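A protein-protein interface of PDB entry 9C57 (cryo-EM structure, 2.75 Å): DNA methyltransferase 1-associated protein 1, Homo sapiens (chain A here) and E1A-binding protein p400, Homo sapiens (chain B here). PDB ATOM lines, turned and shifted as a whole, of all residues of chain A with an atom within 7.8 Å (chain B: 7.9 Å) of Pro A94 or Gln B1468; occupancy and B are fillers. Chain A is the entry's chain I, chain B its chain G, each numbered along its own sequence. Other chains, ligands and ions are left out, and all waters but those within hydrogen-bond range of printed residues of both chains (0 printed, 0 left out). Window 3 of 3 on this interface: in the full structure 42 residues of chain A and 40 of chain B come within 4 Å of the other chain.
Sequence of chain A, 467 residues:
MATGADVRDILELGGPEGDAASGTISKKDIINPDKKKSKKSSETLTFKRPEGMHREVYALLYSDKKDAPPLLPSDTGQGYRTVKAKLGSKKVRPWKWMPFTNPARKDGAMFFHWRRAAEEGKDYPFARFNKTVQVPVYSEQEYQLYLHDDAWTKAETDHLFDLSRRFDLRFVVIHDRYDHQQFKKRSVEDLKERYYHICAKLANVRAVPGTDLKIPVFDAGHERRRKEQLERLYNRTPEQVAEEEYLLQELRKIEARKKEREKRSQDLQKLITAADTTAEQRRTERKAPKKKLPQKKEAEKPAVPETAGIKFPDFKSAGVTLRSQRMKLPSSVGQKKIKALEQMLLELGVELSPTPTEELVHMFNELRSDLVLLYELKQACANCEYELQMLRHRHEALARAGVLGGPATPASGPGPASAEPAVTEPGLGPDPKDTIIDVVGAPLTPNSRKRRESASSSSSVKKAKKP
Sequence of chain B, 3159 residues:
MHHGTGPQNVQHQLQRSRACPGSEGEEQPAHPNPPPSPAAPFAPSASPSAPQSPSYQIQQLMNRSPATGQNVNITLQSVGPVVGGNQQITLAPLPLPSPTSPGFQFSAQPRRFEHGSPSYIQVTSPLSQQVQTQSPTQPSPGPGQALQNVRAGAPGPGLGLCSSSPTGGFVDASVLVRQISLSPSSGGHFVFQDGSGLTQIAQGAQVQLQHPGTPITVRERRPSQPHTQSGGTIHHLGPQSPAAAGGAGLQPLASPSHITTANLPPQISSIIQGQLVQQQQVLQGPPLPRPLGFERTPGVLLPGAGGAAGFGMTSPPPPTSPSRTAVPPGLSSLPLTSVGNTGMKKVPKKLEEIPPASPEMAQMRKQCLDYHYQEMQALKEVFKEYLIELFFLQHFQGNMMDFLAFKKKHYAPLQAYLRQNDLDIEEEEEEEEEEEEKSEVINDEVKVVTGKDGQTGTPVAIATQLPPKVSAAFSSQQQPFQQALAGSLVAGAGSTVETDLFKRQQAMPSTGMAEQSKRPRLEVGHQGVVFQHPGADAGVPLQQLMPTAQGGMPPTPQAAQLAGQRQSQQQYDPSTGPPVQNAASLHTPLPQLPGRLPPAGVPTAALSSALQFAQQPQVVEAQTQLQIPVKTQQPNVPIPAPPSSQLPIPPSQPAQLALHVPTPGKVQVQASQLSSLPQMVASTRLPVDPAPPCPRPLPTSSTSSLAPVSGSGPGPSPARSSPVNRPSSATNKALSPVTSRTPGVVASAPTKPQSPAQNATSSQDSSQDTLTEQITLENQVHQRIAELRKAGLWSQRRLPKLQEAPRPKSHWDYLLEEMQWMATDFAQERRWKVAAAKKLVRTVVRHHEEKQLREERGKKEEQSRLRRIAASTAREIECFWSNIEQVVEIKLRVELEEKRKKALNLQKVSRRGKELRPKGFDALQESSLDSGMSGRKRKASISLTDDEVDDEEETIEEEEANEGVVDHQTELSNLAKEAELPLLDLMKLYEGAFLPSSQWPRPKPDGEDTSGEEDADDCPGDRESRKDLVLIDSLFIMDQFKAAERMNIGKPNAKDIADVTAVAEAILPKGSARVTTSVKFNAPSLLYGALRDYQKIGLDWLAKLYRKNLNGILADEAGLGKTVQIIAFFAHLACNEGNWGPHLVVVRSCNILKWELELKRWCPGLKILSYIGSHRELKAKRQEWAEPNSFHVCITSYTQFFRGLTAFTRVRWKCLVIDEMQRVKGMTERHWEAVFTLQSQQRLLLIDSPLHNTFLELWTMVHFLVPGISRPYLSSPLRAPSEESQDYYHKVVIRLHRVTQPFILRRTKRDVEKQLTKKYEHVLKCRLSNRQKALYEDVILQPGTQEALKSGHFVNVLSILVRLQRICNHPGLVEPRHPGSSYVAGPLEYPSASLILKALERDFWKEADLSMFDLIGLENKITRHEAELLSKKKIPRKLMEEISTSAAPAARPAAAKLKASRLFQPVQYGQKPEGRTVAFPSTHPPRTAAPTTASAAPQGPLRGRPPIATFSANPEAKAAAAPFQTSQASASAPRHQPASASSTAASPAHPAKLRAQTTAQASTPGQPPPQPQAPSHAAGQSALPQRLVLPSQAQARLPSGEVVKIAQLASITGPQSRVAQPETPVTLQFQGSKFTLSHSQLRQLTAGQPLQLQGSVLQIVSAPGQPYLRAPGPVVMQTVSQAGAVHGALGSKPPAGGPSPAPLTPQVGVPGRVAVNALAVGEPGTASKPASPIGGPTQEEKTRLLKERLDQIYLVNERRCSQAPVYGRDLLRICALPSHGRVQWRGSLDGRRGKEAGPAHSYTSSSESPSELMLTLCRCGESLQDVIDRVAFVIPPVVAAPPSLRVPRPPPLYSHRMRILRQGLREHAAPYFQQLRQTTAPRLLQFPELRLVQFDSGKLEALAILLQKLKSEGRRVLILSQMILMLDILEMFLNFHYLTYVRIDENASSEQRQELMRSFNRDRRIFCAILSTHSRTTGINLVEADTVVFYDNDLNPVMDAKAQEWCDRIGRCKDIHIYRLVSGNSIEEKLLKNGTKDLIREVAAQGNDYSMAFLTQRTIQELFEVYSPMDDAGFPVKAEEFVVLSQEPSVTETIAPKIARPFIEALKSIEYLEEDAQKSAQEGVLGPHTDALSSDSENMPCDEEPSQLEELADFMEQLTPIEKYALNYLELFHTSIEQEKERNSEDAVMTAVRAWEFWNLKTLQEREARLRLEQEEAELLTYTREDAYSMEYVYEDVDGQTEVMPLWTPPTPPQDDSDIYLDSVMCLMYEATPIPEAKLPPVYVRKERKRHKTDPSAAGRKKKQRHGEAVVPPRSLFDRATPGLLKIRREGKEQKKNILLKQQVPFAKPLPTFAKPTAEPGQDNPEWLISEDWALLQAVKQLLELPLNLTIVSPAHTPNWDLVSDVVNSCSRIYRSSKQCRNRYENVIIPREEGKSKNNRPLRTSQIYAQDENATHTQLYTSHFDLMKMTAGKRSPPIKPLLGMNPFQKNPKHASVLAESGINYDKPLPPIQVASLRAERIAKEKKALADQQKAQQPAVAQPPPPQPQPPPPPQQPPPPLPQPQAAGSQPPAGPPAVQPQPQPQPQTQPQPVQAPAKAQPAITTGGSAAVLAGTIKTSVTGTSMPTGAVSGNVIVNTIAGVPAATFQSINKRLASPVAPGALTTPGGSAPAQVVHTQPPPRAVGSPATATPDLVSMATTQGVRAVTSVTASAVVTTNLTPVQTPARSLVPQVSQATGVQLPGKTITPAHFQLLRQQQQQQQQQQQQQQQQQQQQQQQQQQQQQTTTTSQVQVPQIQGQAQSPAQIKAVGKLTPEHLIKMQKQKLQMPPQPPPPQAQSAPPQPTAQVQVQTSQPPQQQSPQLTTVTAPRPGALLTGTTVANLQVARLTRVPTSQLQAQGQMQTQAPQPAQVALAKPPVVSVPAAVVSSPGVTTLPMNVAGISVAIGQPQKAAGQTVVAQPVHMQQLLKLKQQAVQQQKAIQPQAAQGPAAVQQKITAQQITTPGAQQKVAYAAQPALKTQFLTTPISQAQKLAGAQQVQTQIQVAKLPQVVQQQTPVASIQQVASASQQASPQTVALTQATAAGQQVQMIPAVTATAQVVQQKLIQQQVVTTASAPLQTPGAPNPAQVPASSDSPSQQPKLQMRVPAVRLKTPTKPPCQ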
ATOM      1  N   SER A  89      13.762  39.135 -35.349  1.00  0.00           N
ATOM      2  CA  SER A  89      12.426  39.542 -35.764  1.00  0.00           C
ATOM      3  C   SER A  89      11.343  38.562 -35.340  1.00  0.00           C
ATOM      4  O   SER A  89      10.159  38.863 -35.524  1.00  0.00           O
ATOM      5  CB  SER A  89      12.391  39.718 -37.281  1.00  0.00           C
ATOM      6  OG  SER A  89      12.964  38.601 -37.933  1.00  0.00           O
ATOM      7  N   LYS A  90      11.704  37.413 -34.781  1.00  0.00           N
ATOM      8  CA  LYS A  90      10.740  36.391 -34.410  1.00  0.00           C
ATOM      9  C   LYS A  90      10.995  35.958 -32.973  1.00  0.00           C
ATOM     10  O   LYS A  90      12.016  36.299 -32.373  1.00  0.00           O
ATOM     11  CB  LYS A  90      10.823  35.195 -35.366  1.00  0.00           C
ATOM     12  CG  LYS A  90      10.916  35.605 -36.828  1.00  0.00           C
ATOM     13  CD  LYS A  90      11.061  34.418 -37.751  1.00  0.00           C
ATOM     14  CE  LYS A  90       9.721  33.788 -38.058  1.00  0.00           C
ATOM     15  NZ  LYS A  90       9.010  34.518 -39.133  1.00  0.00           N
ATOM     16  N   LYS A  91      10.042  35.214 -32.417  1.00  0.00           N
ATOM     17  CA  LYS A  91      10.156  34.721 -31.054  1.00  0.00           C
ATOM     18  C   LYS A  91       9.569  33.320 -30.972  1.00  0.00           C
ATOM     19  O   LYS A  91       8.867  32.861 -31.875  1.00  0.00           O
ATOM     20  CB  LYS A  91       9.472  35.661 -30.050  1.00  0.00           C
ATOM     21  CG  LYS A  91       7.988  35.866 -30.269  1.00  0.00           C
ATOM     22  CD  LYS A  91       7.325  36.434 -29.026  1.00  0.00           C
ATOM     23  CE  LYS A  91       7.935  37.764 -28.621  1.00  0.00           C
ATOM     24  NZ  LYS A  91       7.277  38.331 -27.416  1.00  0.00           N
ATOM     25  N   VAL A  92       9.865  32.651 -29.874  1.00  0.00           N
ATOM     26  CA  VAL A  92       9.637  31.217 -29.741  1.00  0.00           C
ATOM     27  C   VAL A  92       8.232  30.950 -29.229  1.00  0.00           C
ATOM     28  O   VAL A  92       7.627  31.765 -28.526  1.00  0.00           O
ATOM     29  CB  VAL A  92      10.695  30.588 -28.811  1.00  0.00           C
ATOM     30  CG1 VAL A  92      12.068  30.648 -29.452  1.00  0.00           C
ATOM     31  CG2 VAL A  92      10.704  31.288 -27.460  1.00  0.00           C
ATOM     32  N   ARG A  93       7.712  29.785 -29.586  1.00  0.00           N
ATOM     33  CA  ARG A  93       6.429  29.331 -29.073  1.00  0.00           C
ATOM     34  C   ARG A  93       6.624  28.740 -27.682  1.00  0.00           C
ATOM     35  O   ARG A  93       7.423  27.812 -27.526  1.00  0.00           O
ATOM     36  CB  ARG A  93       5.828  28.300 -30.016  1.00  0.00           C
ATOM     37  CG  ARG A  93       5.393  28.888 -31.343  1.00  0.00           C
ATOM     38  CD  ARG A  93       4.955  27.820 -32.321  1.00  0.00           C
ATOM     39  NE  ARG A  93       6.009  27.481 -33.267  1.00  0.00           N
ATOM     40  CZ  ARG A  93       5.812  26.848 -34.414  1.00  0.00           C
ATOM     41  NH1 ARG A  93       4.607  26.454 -34.791  1.00  0.00           N
ATOM     42  NH2 ARG A  93       6.851  26.602 -35.206  1.00  0.00           N
ATOM     43  N   PRO A  94       5.927  29.232 -26.657  1.00  0.00           N
ATOM     44  CA  PRO A  94       6.303  28.875 -25.282  1.00  0.00           C
ATOM     45  C   PRO A  94       6.083  27.409 -24.948  1.00  0.00           C
ATOM     46  O   PRO A  94       4.946  26.944 -24.861  1.00  0.00           O
ATOM     47  CB  PRO A  94       5.405  29.782 -24.430  1.00  0.00           C
ATOM     48  CG  PRO A  94       4.236  30.071 -25.285  1.00  0.00           C
ATOM     49  CD  PRO A  94       4.739  30.101 -26.696  1.00  0.00           C
ATOM     50  N   TRP A  95       7.174  26.679 -24.744  1.00  0.00           N
ATOM     51  CA  TRP A  95       7.101  25.276 -24.373  1.00  0.00           C
ATOM     52  C   TRP A  95       6.826  25.131 -22.882  1.00  0.00           C
ATOM     53  O   TRP A  95       7.225  25.971 -22.070  1.00  0.00           O
ATOM     54  CB  TRP A  95       8.403  24.562 -24.731  1.00  0.00           C
ATOM     55  CG  TRP A  95       8.581  24.338 -26.196  1.00  0.00           C
ATOM     56  CD1 TRP A  95       8.885  25.275 -27.136  1.00  0.00           C
ATOM     57  CD2 TRP A  95       8.479  23.091 -26.892  1.00  0.00           C
ATOM     58  NE1 TRP A  95       8.972  24.693 -28.376  1.00  0.00           N
ATOM     59  CE2 TRP A  95       8.729  23.351 -28.251  1.00  0.00           C
ATOM     60  CE3 TRP A  95       8.200  21.782 -26.496  1.00  0.00           C
ATOM     61  CZ2 TRP A  95       8.706  22.352 -29.216  1.00  0.00           C
ATOM     62  CZ3 TRP A  95       8.178  20.792 -27.455  1.00  0.00           C
ATOM     63  CH2 TRP A  95       8.428  21.081 -28.798  1.00  0.00           C
ATOM     64  N   LYS A  96       6.136  24.049 -22.524  1.00  0.00           N
ATOM     65  CA  LYS A  96       5.777  23.788 -21.139  1.00  0.00           C
ATOM     66  C   LYS A  96       5.910  22.303 -20.846  1.00  0.00           C
ATOM     67  O   LYS A  96       5.788  21.463 -21.742  1.00  0.00           O
ATOM     68  CB  LYS A  96       4.346  24.250 -20.833  1.00  0.00           C
ATOM     69  CG  LYS A  96       4.029  24.332 -19.351  1.00  0.00           C
ATOM     70  CD  LYS A  96       2.772  25.143 -19.087  1.00  0.00           C
ATOM     71  CE  LYS A  96       1.542  24.458 -19.650  1.00  0.00           C
ATOM     72  NZ  LYS A  96       0.284  25.151 -19.262  1.00  0.00           N
ATOM     73  N   TRP A  97       6.169  21.985 -19.579  1.00  0.00           N
ATOM     74  CA  TRP A  97       6.178  20.605 -19.106  1.00  0.00           C
ATOM     75  C   TRP A  97       4.765  20.279 -18.644  1.00  0.00           C
ATOM     76  O   TRP A  97       4.306  20.793 -17.619  1.00  0.00           O
ATOM     77  CB  TRP A  97       7.184  20.415 -17.974  1.00  0.00           C
ATOM     78  CG  TRP A  97       7.725  19.018 -17.857  1.00  0.00           C
ATOM     79  CD1 TRP A  97       7.851  18.099 -18.857  1.00  0.00           C
ATOM     80  CD2 TRP A  97       8.211  18.385 -16.672  1.00  0.00           C
ATOM     81  NE1 TRP A  97       8.388  16.934 -18.368  1.00  0.00           N
ATOM     82  CE2 TRP A  97       8.616  17.084 -17.027  1.00  0.00           C
ATOM     83  CE3 TRP A  97       8.343  18.791 -15.343  1.00  0.00           C
ATOM     84  CZ2 TRP A  97       9.141  16.189 -16.104  1.00  0.00           C
ATOM     85  CZ3 TRP A  97       8.866  17.902 -14.427  1.00  0.00           C
ATOM     86  CH2 TRP A  97       9.259  16.615 -14.811  1.00  0.00           C
ATOM     87  N   TRP A 114       7.645  17.357 -22.479  1.00  0.00           N
ATOM     88  CA  TRP A 114       7.744  18.716 -22.996  1.00  0.00           C
ATOM     89  C   TRP A 114       6.843  18.893 -24.212  1.00  0.00           C
ATOM     90  O   TRP A 114       6.900  18.101 -25.156  1.00  0.00           O
ATOM     91  CB  TRP A 114       9.189  19.038 -23.378  1.00  0.00           C
ATOM     92  CG  TRP A 114      10.068  19.391 -22.222  1.00  0.00           C
ATOM     93  CD1 TRP A 114      11.092  18.645 -21.720  1.00  0.00           C
ATOM     94  CD2 TRP A 114      10.015  20.582 -21.429  1.00  0.00           C
ATOM     95  NE1 TRP A 114      11.675  19.291 -20.662  1.00  0.00           N
ATOM     96  CE2 TRP A 114      11.032  20.484 -20.463  1.00  0.00           C
ATOM     97  CE3 TRP A 114       9.204  21.718 -21.440  1.00  0.00           C
ATOM     98  CZ2 TRP A 114      11.260  21.478 -19.516  1.00  0.00           C
ATOM     99  CZ3 TRP A 114       9.434  22.704 -20.498  1.00  0.00           C
ATOM    100  CH2 TRP A 114      10.453  22.578 -19.551  1.00  0.00           C
ATOM    101  N   ARG A 115       6.022  19.942 -24.194  1.00  0.00           N
ATOM    102  CA  ARG A 115       5.188  20.284 -25.337  1.00  0.00           C
ATOM    103  C   ARG A 115       4.961  21.790 -25.354  1.00  0.00           C
ATOM    104  O   ARG A 115       5.375  22.514 -24.444  1.00  0.00           O
ATOM    105  CB  ARG A 115       3.862  19.517 -25.315  1.00  0.00           C
ATOM    106  CG  ARG A 115       3.578  18.753 -26.604  1.00  0.00           C
ATOM    107  CD  ARG A 115       4.650  17.706 -26.880  1.00  0.00           C
ATOM    108  NE  ARG A 115       4.320  16.834 -28.001  1.00  0.00           N
ATOM    109  CZ  ARG A 115       4.944  15.695 -28.270  1.00  0.00           C
ATOM    110  NH1 ARG A 115       5.921  15.242 -27.502  1.00  0.00           N
ATOM    111  NH2 ARG A 115       4.583  14.994 -29.341  1.00  0.00           N
ATOM    112  N   ARG A 116       4.279  22.254 -26.402  1.00  0.00           N
ATOM    113  CA  ARG A 116       4.334  23.656 -26.800  1.00  0.00           C
ATOM    114  C   ARG A 116       3.381  24.565 -26.037  1.00  0.00           C
ATOM    115  O   ARG A 116       3.362  25.767 -26.313  1.00  0.00           O
ATOM    116  CB  ARG A 116       4.039  23.782 -28.295  1.00  0.00           C
ATOM    117  CG  ARG A 116       5.281  23.908 -29.142  1.00  0.00           C
ATOM    118  CD  ARG A 116       4.942  24.131 -30.594  1.00  0.00           C
ATOM    119  NE  ARG A 116       6.137  24.408 -31.377  1.00  0.00           N
ATOM    120  CZ  ARG A 116       6.220  24.266 -32.692  1.00  0.00           C
ATOM    121  NH1 ARG A 116       5.183  23.880 -33.414  1.00  0.00           N
ATOM    122  NH2 ARG A 116       7.377  24.519 -33.298  1.00  0.00           N
ATOM    123  N   ALA A 117       2.564  24.033 -25.132  1.00  0.00           N
ATOM    124  CA  ALA A 117       1.657  24.854 -24.336  1.00  0.00           C
ATOM    125  C   ALA A 117       0.497  25.377 -25.175  1.00  0.00           C
ATOM    126  O   ALA A 117      -0.438  25.982 -24.641  1.00  0.00           O
ATOM    127  CB  ALA A 117       2.405  26.021 -23.689  1.00  0.00           C
ATOM    128  N   ALA A 118       0.547  25.151 -26.485  1.00  0.00           N
ATOM    129  CA  ALA A 118      -0.596  25.340 -27.361  1.00  0.00           C
ATOM    130  C   ALA A 118      -1.189  24.016 -27.809  1.00  0.00           C
ATOM    131  O   ALA A 118      -2.320  23.990 -28.301  1.00  0.00           O
ATOM    132  CB  ALA A 118      -0.197  26.170 -28.585  1.00  0.00           C
ATOM    133  N   GLU A 119      -0.444  22.923 -27.649  1.00  0.00           N
ATOM    134  CA  GLU A 119      -0.928  21.570 -27.885  1.00  0.00           C
ATOM    135  C   GLU A 119      -1.275  20.852 -26.586  1.00  0.00           C
ATOM    136  O   GLU A 119      -1.499  19.638 -26.596  1.00  0.00           O
ATOM    137  CB  GLU A 119       0.116  20.762 -28.657  1.00  0.00           C
ATOM    138  CG  GLU A 119       0.828  21.498 -29.784  1.00  0.00           C
ATOM    139  CD  GLU A 119      -0.037  22.541 -30.459  1.00  0.00           C
ATOM    140  OE1 GLU A 119      -0.916  22.158 -31.257  1.00  0.00           O
ATOM    141  OE2 GLU A 119       0.181  23.745 -30.213  1.00  0.00           O
ATOM    142  N   GLN B1465       7.085  44.630 -33.484  1.00  0.00           N
ATOM    143  CA  GLN B1465       7.082  43.679 -32.384  1.00  0.00           C
ATOM    144  C   GLN B1465       7.326  42.275 -32.926  1.00  0.00           C
ATOM    145  O   GLN B1465       6.698  41.886 -33.917  1.00  0.00           O
ATOM    146  CB  GLN B1465       5.751  43.753 -31.640  1.00  0.00           C
ATOM    147  CG  GLN B1465       5.818  43.380 -30.182  1.00  0.00           C
ATOM    148  CD  GLN B1465       4.478  43.527 -29.501  1.00  0.00           C
ATOM    149  OE1 GLN B1465       4.232  44.502 -28.794  1.00  0.00           O
ATOM    150  NE2 GLN B1465       3.594  42.563 -29.722  1.00  0.00           N
ATOM    151  N   PRO B1466       8.214  41.486 -32.320  1.00  0.00           N
ATOM    152  CA  PRO B1466       8.544  40.182 -32.904  1.00  0.00           C
ATOM    153  C   PRO B1466       7.320  39.290 -33.032  1.00  0.00           C
ATOM    154  O   PRO B1466       6.368  39.381 -32.254  1.00  0.00           O
ATOM    155  CB  PRO B1466       9.563  39.599 -31.919  1.00  0.00           C
ATOM    156  CG  PRO B1466      10.154  40.773 -31.253  1.00  0.00           C
ATOM    157  CD  PRO B1466       9.052  41.778 -31.144  1.00  0.00           C
ATOM    158  N   VAL B1467       7.353  38.426 -34.040  1.00  0.00           N
ATOM    159  CA  VAL B1467       6.250  37.528 -34.356  1.00  0.00           C
ATOM    160  C   VAL B1467       6.607  36.125 -33.891  1.00  0.00           C
ATOM    161  O   VAL B1467       7.713  35.635 -34.149  1.00  0.00           O
ATOM    162  CB  VAL B1467       5.936  37.538 -35.860  1.00  0.00           C
ATOM    163  CG1 VAL B1467       4.766  36.622 -36.162  1.00  0.00           C
ATOM    164  CG2 VAL B1467       5.645  38.950 -36.331  1.00  0.00           C
ATOM    165  N   GLN B1468       5.673  35.482 -33.204  1.00  0.00           N
ATOM    166  CA  GLN B1468       5.858  34.101 -32.790  1.00  0.00           C
ATOM    167  C   GLN B1468       5.952  33.196 -34.012  1.00  0.00           C
ATOM    168  O   GLN B1468       5.202  33.355 -34.978  1.00  0.00           O
ATOM    169  CB  GLN B1468       4.693  33.675 -31.902  1.00  0.00           C
ATOM    170  CG  GLN B1468       4.864  32.345 -31.224  1.00  0.00           C
ATOM    171  CD  GLN B1468       3.771  32.087 -30.218  1.00  0.00           C
ATOM    172  OE1 GLN B1468       2.908  31.237 -30.426  1.00  0.00           O
ATOM    173  NE2 GLN B1468       3.789  32.837 -29.125  1.00  0.00           N
ATOM    174  N   TYR B1469       6.881  32.246 -33.969  1.00  0.00           N
ATOM    175  CA  TYR B1469       7.080  31.357 -35.104  1.00  0.00           C
ATOM    176  C   TYR B1469       5.778  30.650 -35.455  1.00  0.00           C
ATOM    177  O   TYR B1469       5.103  30.095 -34.584  1.00  0.00           O
ATOM    178  CB  TYR B1469       8.168  30.330 -34.790  1.00  0.00           C
ATOM    179  CG  TYR B1469       9.576  30.813 -35.060  1.00  0.00           C
ATOM    180  CD1 TYR B1469      10.148  30.673 -36.316  1.00  0.00           C
ATOM    181  CD2 TYR B1469      10.334  31.400 -34.061  1.00  0.00           C
ATOM    182  CE1 TYR B1469      11.426  31.107 -36.566  1.00  0.00           C
ATOM    183  CE2 TYR B1469      11.614  31.837 -34.303  1.00  0.00           C
ATOM    184  CZ  TYR B1469      12.156  31.688 -35.556  1.00  0.00           C
ATOM    185  OH  TYR B1469      13.436  32.122 -35.800  1.00  0.00           O
ATOM    186  N   GLY B1470       5.431  30.671 -36.737  1.00  0.00           N
ATOM    187  CA  GLY B1470       4.199  30.100 -37.222  1.00  0.00           C
ATOM    188  C   GLY B1470       3.080  31.101 -37.414  1.00  0.00           C
ATOM    189  O   GLY B1470       2.184  30.857 -38.227  1.00  0.00           O
ATOM    190  N   GLN B1471       3.107  32.217 -36.690  1.00  0.00           N
ATOM    191  CA  GLN B1471       2.151  33.287 -36.922  1.00  0.00           C
ATOM    192  C   GLN B1471       2.576  34.094 -38.138  1.00  0.00           C
ATOM    193  O   GLN B1471       3.752  34.440 -38.285  1.00  0.00           O
ATOM    194  CB  GLN B1471       2.048  34.194 -35.699  1.00  0.00           C
ATOM    195  CG  GLN B1471       1.299  33.582 -34.541  1.00  0.00           C
ATOM    196  CD  GLN B1471       1.084  34.569 -33.420  1.00  0.00           C
ATOM    197  OE1 GLN B1471       1.575  35.694 -33.469  1.00  0.00           O
ATOM    198  NE2 GLN B1471       0.348  34.154 -32.398  1.00  0.00           N
ATOM    199  N   LYS B1472       1.624  34.387 -39.011  1.00  0.00           N
ATOM    200  CA  LYS B1472       1.943  35.122 -40.222  1.00  0.00           C
ATOM    201  C   LYS B1472       2.412  36.528 -39.859  1.00  0.00           C
ATOM    202  O   LYS B1472       1.836  37.153 -38.960  1.00  0.00           O
ATOM    203  CB  LYS B1472       0.725  35.193 -41.141  1.00  0.00           C
ATOM    204  CG  LYS B1472       0.215  33.840 -41.608  1.00  0.00           C
ATOM    205  CD  LYS B1472       1.337  32.960 -42.141  1.00  0.00           C
ATOM    206  CE  LYS B1472       0.881  32.066 -43.285  1.00  0.00           C
ATOM    207  NZ  LYS B1472       0.220  32.818 -44.388  1.00  0.00           N
ATOM    208  N   PRO B1473       3.441  37.057 -40.518  1.00  0.00           N
ATOM    209  CA  PRO B1473       3.933  38.387 -40.144  1.00  0.00           C
ATOM    210  C   PRO B1473       2.911  39.468 -40.460  1.00  0.00           C
ATOM    211  O   PRO B1473       2.489  39.633 -41.606  1.00  0.00           O
ATOM    212  CB  PRO B1473       5.204  38.550 -40.988  1.00  0.00           C
ATOM    213  CG  PRO B1473       5.513  37.202 -41.526  1.00  0.00           C
ATOM    214  CD  PRO B1473       4.224  36.478 -41.620  1.00  0.00           C
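The backbone carbonyl oxygen (O) of Pro A94 lies close to the backbone carbonyl oxygen (O) of Arg A116 (2.5 Å).
Of the 9 printed residues of chain B, 4 touch a printed residue of chain A.
Printed residues of chain B that touch a printed residue of chain A: Pro B1466, Val B1467, Gln B1468 and Tyr B1469.
Hydrophobic or aromatic side chains of chain B within 4 Å of the printed part of chain A: Pro B1466 and Tyr B1469.
Along chain B the printed residues that touch a printed residue of chain A span positions 1466 to 1469.
Of the 15 printed residues of chain A, 6 touch a printed residue of chain B.
Printed residues of chain A that touch a printed residue of chain B: Ser A89, Lys A90, Lys A91, Val A92, Arg A93 and Pro A94.
Among the printed residues, no Asp or Glu carboxylate lies within 4 Å of a Lys or Arg side-chain nitrogen of the other chain.
The backbone NH (N) of Val B1467 sits at hydrogen-bond distance from the backbone carbonyl oxygen (O) of Ser A89 (3.2 Å).
The backbone carbonyl oxygen (O) of Val B1467 lies within hydrogen-bond range of the backbone NH (N) of Lys A91.
The backbone carbonyl oxygen (O) of Lys A91 is in hydrogen-bond range of the backbone NH (N) of Tyr B1469, 3.0 Å away.
The backbone carbonyl oxygen of Tyr B1469 is in hydrogen-bond range of the guanidinium group of Arg A93.
Of chain A, only Lys A91 (3.4 Å), Val A92 (3.9 Å), Arg A93 (3.5 Å) and Pro A94 (3.8 Å) come within 4 Å of Gln B1468.
Printed residues of chain A within 4 Å of Pro B1466: Ser A89.
Of the printed residues of chain B, Arg A93 touches Gln B1468 and Tyr B1469.
Printed residues of chain B within 4 Å of Lys A90: Val B1467 and Tyr B1469.
Of the printed residues of chain B, Ser A89 touches Pro B1466 and Val B1467.
Printed residues of chain A within 4 Å of Val B1467: Ser A89, Lys A90 and Lys A91.
The nearest printed residue of chain B that does not touch Arg A93 is Gly B1470 (4.4 Å).
Ser A89 touches Pro B1466 (O to CA, 3.3 Å).
Lys A90 touches Val B1467.
CE1 of Tyr B1469 touches CE of Lys A90 (3.5 Å).
O of Lys A91 touches CA of Gln B1468, at 3.4 Å.
Val A92 touches Gln B1468 (O to CG, 3.9 Å).
CG of Arg A93 touches CG of Gln B1468, 3.5 Å away.
CD of Pro A94 touches NE2 of Gln B1468, at 3.8 Å.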
